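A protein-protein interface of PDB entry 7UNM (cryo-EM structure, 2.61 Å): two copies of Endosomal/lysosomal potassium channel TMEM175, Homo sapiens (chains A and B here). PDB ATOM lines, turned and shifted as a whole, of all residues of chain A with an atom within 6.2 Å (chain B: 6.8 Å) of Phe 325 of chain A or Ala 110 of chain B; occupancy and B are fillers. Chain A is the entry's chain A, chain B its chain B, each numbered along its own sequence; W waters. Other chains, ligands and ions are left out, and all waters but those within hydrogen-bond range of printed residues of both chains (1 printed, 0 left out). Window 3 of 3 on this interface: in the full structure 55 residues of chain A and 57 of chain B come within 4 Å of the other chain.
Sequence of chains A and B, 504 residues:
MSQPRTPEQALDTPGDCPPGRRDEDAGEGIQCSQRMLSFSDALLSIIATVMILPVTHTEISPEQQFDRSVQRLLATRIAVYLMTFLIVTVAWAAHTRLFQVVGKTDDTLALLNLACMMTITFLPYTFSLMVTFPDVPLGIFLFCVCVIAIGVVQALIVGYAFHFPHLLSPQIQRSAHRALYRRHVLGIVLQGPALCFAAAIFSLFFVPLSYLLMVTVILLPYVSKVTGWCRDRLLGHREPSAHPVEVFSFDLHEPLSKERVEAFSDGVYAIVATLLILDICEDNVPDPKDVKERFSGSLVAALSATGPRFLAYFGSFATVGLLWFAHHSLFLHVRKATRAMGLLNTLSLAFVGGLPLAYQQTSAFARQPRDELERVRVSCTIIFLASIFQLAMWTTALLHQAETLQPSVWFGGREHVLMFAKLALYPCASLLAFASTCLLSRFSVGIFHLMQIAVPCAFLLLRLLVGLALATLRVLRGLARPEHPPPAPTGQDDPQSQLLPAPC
NZ of Lys 422 of chain A is in salt-bridge range of OD2 of Asp 107 of chain B, 3.4 Å away.
The side-chain hydroxyl of Thr 105 of chain B sits at hydrogen-bond distance from the side-chain sulfur of Met 36 of chain B, at 3.3 Å.
The backbone carbonyl oxygen (O) of Phe 325 of chain A sits at hydrogen-bond distance from the side-chain hydroxyl (OG) of Ser 329 of chain A.
NE2 of Gln 31 of chain B lies within hydrogen-bond range of OD1 of Asp 107 of chain B, at 2.8 Å.
The side-chain hydroxyl (OG) of Ser 329 of chain A is in hydrogen-bond range of the side-chain amino group (NZ) of Lys 422 of chain A, 3.3 Å away.
O of Gly 321 of chain A touches CD1 of Leu 114 of chain B (3.3 Å).
Leu 111 of chain B touches Leu 322 of chain A (CD2 to CD2, 3.6 Å).
Met 36 of chain B touches Trp 324 of chain A.
Phe 325 of chain A touches Asp 107 of chain B.
CE1 of Phe 325 of chain A touches CB of Ala 110 of chain B (3.8 Å).
Phe 325 of chain A touches Leu 114 of chain B.
Of the printed residues of chain B, Gly 321 of chain A touches Leu 114 (3.3 Å).
Printed residues of chain B within 4 Å of Phe 325 of chain A: Asp 107, Ala 110 and Leu 114.
His 327 of chain A touches none of the printed residues of chain B.
Of the printed residues of chain B, Lys 422 of chain A touches Asp 107 (3.4 Å).
Printed residues of chain A within 4 Å of Asp 107 of chain B: Phe 325 and Lys 422.
Of chain A, only Phe 325 comes within 4 Å of Ala 110 of chain B.
Of the printed residues of chain A, Leu 111 of chain B touches Leu 322 (3.6 Å).
Printed residues of chain A that touch a printed residue of chain B: Gly 321, Leu 322, Trp 324, Phe 325 and Lys 422.
Of the 14 printed residues of chain B, 5 touch a printed residue of chain A.
Hydrophobic or aromatic side chains of chain B within 4 Å of the printed part of chain A: Ala 110, Leu 111 and Leu 114.
Among the printed residues, Asp or Glu carboxylates within 4 Å of a Lys or Arg side-chain nitrogen of the other chain: Lys 422 of chain A with Asp 107 of chain B (3.4 Å).
No position is printed for both chains.
Of the 7 pairs that touch across the chains among the printed residues, none has its exchanged pair printed and touching as well.
Water W1 lies within hydrogen-bond range of the side-chain carboxylate (OD1) of Asp 107 of chain B (2.9 Å), the side-chain amide oxygen (OE1) of Gln 31 of chain B (3.1 Å) and the side-chain hydroxyl (OG) of Ser 329 of chain A (3.1 Å).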
ATOM      1  N   VAL A 320     -18.690  -5.853  24.212  1.00  0.00           N
ATOM      2  CA  VAL A 320     -19.296  -4.541  24.023  1.00  0.00           C
ATOM      3  C   VAL A 320     -19.752  -4.379  22.580  1.00  0.00           C
ATOM      4  O   VAL A 320     -20.906  -4.024  22.310  1.00  0.00           O
ATOM      5  CB  VAL A 320     -18.311  -3.431  24.431  1.00  0.00           C
ATOM      6  CG1 VAL A 320     -18.959  -2.062  24.293  1.00  0.00           C
ATOM      7  CG2 VAL A 320     -17.820  -3.649  25.853  1.00  0.00           C
ATOM      8  N   GLY A 321     -18.867  -4.690  21.631  1.00  0.00           N
ATOM      9  CA  GLY A 321     -19.178  -4.440  20.234  1.00  0.00           C
ATOM     10  C   GLY A 321     -20.415  -5.181  19.772  1.00  0.00           C
ATOM     11  O   GLY A 321     -21.206  -4.658  18.983  1.00  0.00           O
ATOM     12  N   LEU A 322     -20.596  -6.412  20.249  1.00  0.00           N
ATOM     13  CA  LEU A 322     -21.794  -7.160  19.895  1.00  0.00           C
ATOM     14  C   LEU A 322     -23.025  -6.610  20.602  1.00  0.00           C
ATOM     15  O   LEU A 322     -24.110  -6.577  20.011  1.00  0.00           O
ATOM     16  CB  LEU A 322     -21.601  -8.637  20.221  1.00  0.00           C
ATOM     17  CG  LEU A 322     -20.644  -9.374  19.283  1.00  0.00           C
ATOM     18  CD1 LEU A 322     -20.234 -10.704  19.882  1.00  0.00           C
ATOM     19  CD2 LEU A 322     -21.269  -9.571  17.912  1.00  0.00           C
ATOM     20  N   LEU A 323     -22.883  -6.160  21.851  1.00  0.00           N
ATOM     21  CA  LEU A 323     -24.019  -5.543  22.527  1.00  0.00           C
ATOM     22  C   LEU A 323     -24.538  -4.363  21.720  1.00  0.00           C
ATOM     23  O   LEU A 323     -25.729  -4.290  21.396  1.00  0.00           O
ATOM     24  CB  LEU A 323     -23.621  -5.103  23.936  1.00  0.00           C
ATOM     25  CG  LEU A 323     -23.770  -6.158  25.034  1.00  0.00           C
ATOM     26  CD1 LEU A 323     -23.039  -5.722  26.287  1.00  0.00           C
ATOM     27  CD2 LEU A 323     -25.236  -6.424  25.338  1.00  0.00           C
ATOM     28  N   TRP A 324     -23.642  -3.447  21.346  1.00  0.00           N
ATOM     29  CA  TRP A 324     -24.023  -2.371  20.442  1.00  0.00           C
ATOM     30  C   TRP A 324     -24.682  -2.929  19.190  1.00  0.00           C
ATOM     31  O   TRP A 324     -25.720  -2.425  18.748  1.00  0.00           O
ATOM     32  CB  TRP A 324     -22.796  -1.534  20.072  1.00  0.00           C
ATOM     33  CG  TRP A 324     -23.080  -0.499  19.030  1.00  0.00           C
ATOM     34  CD1 TRP A 324     -23.528   0.772  19.237  1.00  0.00           C
ATOM     35  CD2 TRP A 324     -22.945  -0.648  17.612  1.00  0.00           C
ATOM     36  NE1 TRP A 324     -23.679   1.423  18.039  1.00  0.00           N
ATOM     37  CE2 TRP A 324     -23.328   0.572  17.025  1.00  0.00           C
ATOM     38  CE3 TRP A 324     -22.538  -1.697  16.781  1.00  0.00           C
ATOM     39  CZ2 TRP A 324     -23.316   0.773  15.650  1.00  0.00           C
ATOM     40  CZ3 TRP A 324     -22.528  -1.495  15.418  1.00  0.00           C
ATOM     41  CH2 TRP A 324     -22.912  -0.270  14.865  1.00  0.00           C
ATOM     42  N   PHE A 325     -24.108  -3.992  18.622  1.00  0.00           N
ATOM     43  CA  PHE A 325     -24.676  -4.568  17.409  1.00  0.00           C
ATOM     44  C   PHE A 325     -26.131  -4.954  17.625  1.00  0.00           C
ATOM     45  O   PHE A 325     -26.969  -4.766  16.736  1.00  0.00           O
ATOM     46  CB  PHE A 325     -23.859  -5.780  16.965  1.00  0.00           C
ATOM     47  CG  PHE A 325     -24.471  -6.535  15.823  1.00  0.00           C
ATOM     48  CD1 PHE A 325     -24.431  -6.025  14.538  1.00  0.00           C
ATOM     49  CD2 PHE A 325     -25.091  -7.753  16.035  1.00  0.00           C
ATOM     50  CE1 PHE A 325     -24.995  -6.715  13.489  1.00  0.00           C
ATOM     51  CE2 PHE A 325     -25.657  -8.448  14.988  1.00  0.00           C
ATOM     52  CZ  PHE A 325     -25.608  -7.928  13.714  1.00  0.00           C
ATOM     53  N   ALA A 326     -26.453  -5.494  18.801  1.00  0.00           N
ATOM     54  CA  ALA A 326     -27.850  -5.774  19.109  1.00  0.00           C
ATOM     55  C   ALA A 326     -28.653  -4.482  19.150  1.00  0.00           C
ATOM     56  O   ALA A 326     -29.667  -4.346  18.455  1.00  0.00           O
ATOM     57  CB  ALA A 326     -27.953  -6.524  20.436  1.00  0.00           C
ATOM     58  N   HIS A 327     -28.186  -3.504  19.928  1.00  0.00           N
ATOM     59  CA  HIS A 327     -28.870  -2.218  19.994  1.00  0.00           C
ATOM     60  C   HIS A 327     -29.036  -1.630  18.602  1.00  0.00           C
ATOM     61  O   HIS A 327     -30.154  -1.317  18.172  1.00  0.00           O
ATOM     62  CB  HIS A 327     -28.082  -1.268  20.897  1.00  0.00           C
ATOM     63  CG  HIS A 327     -28.867  -0.088  21.373  1.00  0.00           C
ATOM     64  ND1 HIS A 327     -29.104   1.016  20.585  1.00  0.00           N
ATOM     65  CD2 HIS A 327     -29.468   0.163  22.559  1.00  0.00           C
ATOM     66  CE1 HIS A 327     -29.816   1.897  21.263  1.00  0.00           C
ATOM     67  NE2 HIS A 327     -30.051   1.402  22.464  1.00  0.00           N
ATOM     68  N   HIS A 328     -27.933  -1.529  17.859  1.00  0.00           N
ATOM     69  CA  HIS A 328     -27.985  -1.014  16.498  1.00  0.00           C
ATOM     70  C   HIS A 328     -29.045  -1.735  15.681  1.00  0.00           C
ATOM     71  O   HIS A 328     -29.768  -1.112  14.897  1.00  0.00           O
ATOM     72  CB  HIS A 328     -26.611  -1.155  15.844  1.00  0.00           C
ATOM     73  CG  HIS A 328     -26.623  -0.959  14.360  1.00  0.00           C
ATOM     74  ND1 HIS A 328     -26.710   0.286  13.774  1.00  0.00           N
ATOM     75  CD2 HIS A 328     -26.557  -1.848  13.343  1.00  0.00           C
ATOM     76  CE1 HIS A 328     -26.698   0.154  12.461  1.00  0.00           C
ATOM     77  NE2 HIS A 328     -26.606  -1.132  12.173  1.00  0.00           N
ATOM     78  N   SER A 329     -29.156  -3.053  15.854  1.00  0.00           N
ATOM     79  CA  SER A 329     -30.163  -3.797  15.109  1.00  0.00           C
ATOM     80  C   SER A 329     -31.566  -3.376  15.518  1.00  0.00           C
ATOM     81  O   SER A 329     -32.395  -3.043  14.664  1.00  0.00           O
ATOM     82  CB  SER A 329     -29.968  -5.296  15.324  1.00  0.00           C
ATOM     83  OG  SER A 329     -28.730  -5.729  14.797  1.00  0.00           O
ATOM     84  N   LEU A 330     -31.836  -3.342  16.824  1.00  0.00           N
ATOM     85  CA  LEU A 330     -33.196  -3.093  17.285  1.00  0.00           C
ATOM     86  C   LEU A 330     -33.723  -1.777  16.734  1.00  0.00           C
ATOM     87  O   LEU A 330     -34.796  -1.733  16.121  1.00  0.00           O
ATOM     88  CB  LEU A 330     -33.234  -3.096  18.814  1.00  0.00           C
ATOM     89  CG  LEU A 330     -34.518  -2.599  19.483  1.00  0.00           C
ATOM     90  CD1 LEU A 330     -35.734  -3.351  18.967  1.00  0.00           C
ATOM     91  CD2 LEU A 330     -34.407  -2.736  20.990  1.00  0.00           C
ATOM     92  N   LYS A 422     -31.620 -12.472  18.375  1.00  0.00           N
ATOM     93  CA  LYS A 422     -30.478 -11.573  18.459  1.00  0.00           C
ATOM     94  C   LYS A 422     -30.452 -10.845  19.795  1.00  0.00           C
ATOM     95  O   LYS A 422     -29.383 -10.651  20.385  1.00  0.00           O
ATOM     96  CB  LYS A 422     -30.529 -10.576  17.302  1.00  0.00           C
ATOM     97  CG  LYS A 422     -29.204  -9.932  16.960  1.00  0.00           C
ATOM     98  CD  LYS A 422     -29.357  -8.915  15.840  1.00  0.00           C
ATOM     99  CE  LYS A 422     -29.694  -9.579  14.515  1.00  0.00           C
ATOM    100  NZ  LYS A 422     -29.749  -8.596  13.399  1.00  0.00           N
ATOM    101  N   PHE A 459     -23.670 -15.059  16.928  1.00  0.00           N
ATOM    102  CA  PHE A 459     -24.124 -13.871  16.212  1.00  0.00           C
ATOM    103  C   PHE A 459     -23.802 -13.970  14.728  1.00  0.00           C
ATOM    104  O   PHE A 459     -24.624 -13.600  13.882  1.00  0.00           O
ATOM    105  CB  PHE A 459     -23.482 -12.621  16.812  1.00  0.00           C
ATOM    106  CG  PHE A 459     -24.310 -11.966  17.878  1.00  0.00           C
ATOM    107  CD1 PHE A 459     -25.410 -11.198  17.544  1.00  0.00           C
ATOM    108  CD2 PHE A 459     -23.985 -12.116  19.214  1.00  0.00           C
ATOM    109  CE1 PHE A 459     -26.170 -10.594  18.522  1.00  0.00           C
ATOM    110  CE2 PHE A 459     -24.742 -11.513  20.196  1.00  0.00           C
ATOM    111  CZ  PHE A 459     -25.835 -10.753  19.850  1.00  0.00           C
ATOM    112  N   GLN B  31     -29.740  -2.532   5.169  1.00  0.00           N
ATOM    113  CA  GLN B  31     -29.784  -1.572   6.260  1.00  0.00           C
ATOM    114  C   GLN B  31     -29.047  -0.293   5.881  1.00  0.00           C
ATOM    115  O   GLN B  31     -28.161  -0.294   5.025  1.00  0.00           O
ATOM    116  CB  GLN B  31     -29.166  -2.167   7.528  1.00  0.00           C
ATOM    117  CG  GLN B  31     -29.643  -3.577   7.863  1.00  0.00           C
ATOM    118  CD  GLN B  31     -28.688  -4.320   8.778  1.00  0.00           C
ATOM    119  OE1 GLN B  31     -27.603  -3.831   9.095  1.00  0.00           O
ATOM    120  NE2 GLN B  31     -29.087  -5.512   9.203  1.00  0.00           N
ATOM    121  N   MET B  36     -23.844   3.172  11.800  1.00  0.00           N
ATOM    122  CA  MET B  36     -22.607   2.407  11.909  1.00  0.00           C
ATOM    123  C   MET B  36     -21.396   3.297  11.663  1.00  0.00           C
ATOM    124  O   MET B  36     -20.396   3.221  12.389  1.00  0.00           O
ATOM    125  CB  MET B  36     -22.638   1.243  10.919  1.00  0.00           C
ATOM    126  CG  MET B  36     -21.494   0.260  11.063  1.00  0.00           C
ATOM    127  SD  MET B  36     -21.501  -0.974   9.753  1.00  0.00           S
ATOM    128  CE  MET B  36     -20.771  -0.048   8.409  1.00  0.00           C
ATOM    129  N   PHE B  99     -16.074   2.792   3.012  1.00  0.00           N
ATOM    130  CA  PHE B  99     -17.520   2.814   3.178  1.00  0.00           C
ATOM    131  C   PHE B  99     -18.192   3.943   2.408  1.00  0.00           C
ATOM    132  O   PHE B  99     -19.417   4.075   2.476  1.00  0.00           O
ATOM    133  CB  PHE B  99     -17.876   2.874   4.663  1.00  0.00           C
ATOM    134  CG  PHE B  99     -17.871   1.525   5.319  1.00  0.00           C
ATOM    135  CD1 PHE B  99     -18.868   0.606   5.043  1.00  0.00           C
ATOM    136  CD2 PHE B  99     -16.855   1.159   6.180  1.00  0.00           C
ATOM    137  CE1 PHE B  99     -18.860  -0.641   5.629  1.00  0.00           C
ATOM    138  CE2 PHE B  99     -16.844  -0.088   6.769  1.00  0.00           C
ATOM    139  CZ  PHE B  99     -17.846  -0.988   6.493  1.00  0.00           C
ATOM    140  N   THR B 105     -25.081  -1.305   4.249  1.00  0.00           N
ATOM    141  CA  THR B 105     -24.519  -2.189   5.257  1.00  0.00           C
ATOM    142  C   THR B 105     -25.415  -3.406   5.438  1.00  0.00           C
ATOM    143  O   THR B 105     -26.522  -3.485   4.899  1.00  0.00           O
ATOM    144  CB  THR B 105     -24.330  -1.469   6.601  1.00  0.00           C
ATOM    145  OG1 THR B 105     -23.507  -2.267   7.459  1.00  0.00           O
ATOM    146  CG2 THR B 105     -25.665  -1.225   7.277  1.00  0.00           C
ATOM    147  N   ASP B 106     -24.908  -4.361   6.212  1.00  0.00           N
ATOM    148  CA  ASP B 106     -25.585  -5.626   6.446  1.00  0.00           C
ATOM    149  C   ASP B 106     -25.054  -6.210   7.745  1.00  0.00           C
ATOM    150  O   ASP B 106     -24.035  -5.760   8.275  1.00  0.00           O
ATOM    151  CB  ASP B 106     -25.373  -6.591   5.272  1.00  0.00           C
ATOM    152  CG  ASP B 106     -26.151  -7.879   5.425  1.00  0.00           C
ATOM    153  OD1 ASP B 106     -27.286  -7.829   5.944  1.00  0.00           O
ATOM    154  OD2 ASP B 106     -25.630  -8.939   5.024  1.00  0.00           O
ATOM    155  N   ASP B 107     -25.765  -7.212   8.269  1.00  0.00           N
ATOM    156  CA  ASP B 107     -25.336  -7.853   9.507  1.00  0.00           C
ATOM    157  C   ASP B 107     -23.887  -8.315   9.410  1.00  0.00           C
ATOM    158  O   ASP B 107     -23.060  -8.010  10.279  1.00  0.00           O
ATOM    159  CB  ASP B 107     -26.255  -9.033   9.826  1.00  0.00           C
ATOM    160  CG  ASP B 107     -27.614  -8.596  10.336  1.00  0.00           C
ATOM    161  OD1 ASP B 107     -27.743  -7.436  10.781  1.00  0.00           O
ATOM    162  OD2 ASP B 107     -28.557  -9.412  10.291  1.00  0.00           O
ATOM    163  N   THR B 108     -23.560  -9.048   8.344  1.00  0.00           N
ATOM    164  CA  THR B 108     -22.185  -9.491   8.150  1.00  0.00           C
ATOM    165  C   THR B 108     -21.246  -8.304   7.989  1.00  0.00           C
ATOM    166  O   THR B 108     -20.146  -8.291   8.553  1.00  0.00           O
ATOM    167  CB  THR B 108     -22.098 -10.410   6.932  1.00  0.00           C
ATOM    168  OG1 THR B 108     -22.984 -11.523   7.106  1.00  0.00           O
ATOM    169  CG2 THR B 108     -20.678 -10.922   6.745  1.00  0.00           C
ATOM    170  N   LEU B 109     -21.663  -7.296   7.222  1.00  0.00           N
ATOM    171  CA  LEU B 109     -20.835  -6.108   7.054  1.00  0.00           C
ATOM    172  C   LEU B 109     -20.662  -5.367   8.372  1.00  0.00           C
ATOM    173  O   LEU B 109     -19.582  -4.843   8.658  1.00  0.00           O
ATOM    174  CB  LEU B 109     -21.440  -5.186   5.996  1.00  0.00           C
ATOM    175  CG  LEU B 109     -21.172  -5.562   4.537  1.00  0.00           C
ATOM    176  CD1 LEU B 109     -21.989  -4.688   3.606  1.00  0.00           C
ATOM    177  CD2 LEU B 109     -19.692  -5.450   4.213  1.00  0.00           C
ATOM    178  N   ALA B 110     -21.718  -5.305   9.187  1.00  0.00           N
ATOM    179  CA  ALA B 110     -21.600  -4.656  10.490  1.00  0.00           C
ATOM    180  C   ALA B 110     -20.609  -5.388  11.386  1.00  0.00           C
ATOM    181  O   ALA B 110     -19.786  -4.758  12.061  1.00  0.00           O
ATOM    182  CB  ALA B 110     -22.971  -4.574  11.158  1.00  0.00           C
ATOM    183  N   LEU B 111     -20.668  -6.721  11.406  1.00  0.00           N
ATOM    184  CA  LEU B 111     -19.722  -7.479  12.220  1.00  0.00           C
ATOM    185  C   LEU B 111     -18.294  -7.316  11.708  1.00  0.00           C
ATOM    186  O   LEU B 111     -17.350  -7.199  12.501  1.00  0.00           O
ATOM    187  CB  LEU B 111     -20.122  -8.953  12.248  1.00  0.00           C
ATOM    188  CG  LEU B 111     -21.467  -9.256  12.915  1.00  0.00           C
ATOM    189  CD1 LEU B 111     -21.787 -10.736  12.814  1.00  0.00           C
ATOM    190  CD2 LEU B 111     -21.475  -8.803  14.364  1.00  0.00           C
ATOM    191  N   LEU B 112     -18.115  -7.304  10.385  1.00  0.00           N
ATOM    192  CA  LEU B 112     -16.785  -7.090   9.824  1.00  0.00           C
ATOM    193  C   LEU B 112     -16.264  -5.698  10.166  1.00  0.00           C
ATOM    194  O   LEU B 112     -15.072  -5.521  10.444  1.00  0.00           O
ATOM    195  CB  LEU B 112     -16.817  -7.297   8.311  1.00  0.00           C
ATOM    196  CG  LEU B 112     -17.002  -8.742   7.843  1.00  0.00           C
ATOM    197  CD1 LEU B 112     -17.239  -8.791   6.343  1.00  0.00           C
ATOM    198  CD2 LEU B 112     -15.803  -9.593   8.222  1.00  0.00           C
ATOM    199  N   ASN B 113     -17.143  -4.696  10.147  1.00  0.00           N
ATOM    200  CA  ASN B 113     -16.744  -3.353  10.550  1.00  0.00           C
ATOM    201  C   ASN B 113     -16.346  -3.321  12.019  1.00  0.00           C
ATOM    202  O   ASN B 113     -15.405  -2.617  12.398  1.00  0.00           O
ATOM    203  CB  ASN B 113     -17.881  -2.367  10.280  1.00  0.00           C
ATOM    204  CG  ASN B 113     -17.468  -0.930  10.515  1.00  0.00           C
ATOM    205  OD1 ASN B 113     -16.558  -0.424   9.864  1.00  0.00           O
ATOM    206  ND2 ASN B 113     -18.134  -0.265  11.450  1.00  0.00           N
ATOM    207  N   LEU B 114     -17.059  -4.066  12.864  1.00  0.00           N
ATOM    208  CA  LEU B 114     -16.673  -4.152  14.269  1.00  0.00           C
ATOM    209  C   LEU B 114     -15.292  -4.778  14.420  1.00  0.00           C
ATOM    210  O   LEU B 114     -14.481  -4.326  15.236  1.00  0.00           O
ATOM    211  CB  LEU B 114     -17.710  -4.955  15.051  1.00  0.00           C
ATOM    212  CG  LEU B 114     -18.982  -4.201  15.436  1.00  0.00           C
ATOM    213  CD1 LEU B 114     -20.059  -5.174  15.883  1.00  0.00           C
ATOM    214  CD2 LEU B 114     -18.690  -3.178  16.523  1.00  0.00           C
ATOM    215  N   ALA B 115     -15.011  -5.828  13.646  1.00  0.00           N
ATOM    216  CA  ALA B 115     -13.684  -6.437  13.681  1.00  0.00           C
ATOM    217  C   ALA B 115     -12.611  -5.448  13.237  1.00  0.00           C
ATOM    218  O   ALA B 115     -11.529  -5.376  13.835  1.00  0.00           O
ATOM    219  CB  ALA B 115     -13.657  -7.684  12.798  1.00  0.00           C
HETATM  220  O   HOH W   1     -27.532  -4.796  12.062  1.00  0.00           O
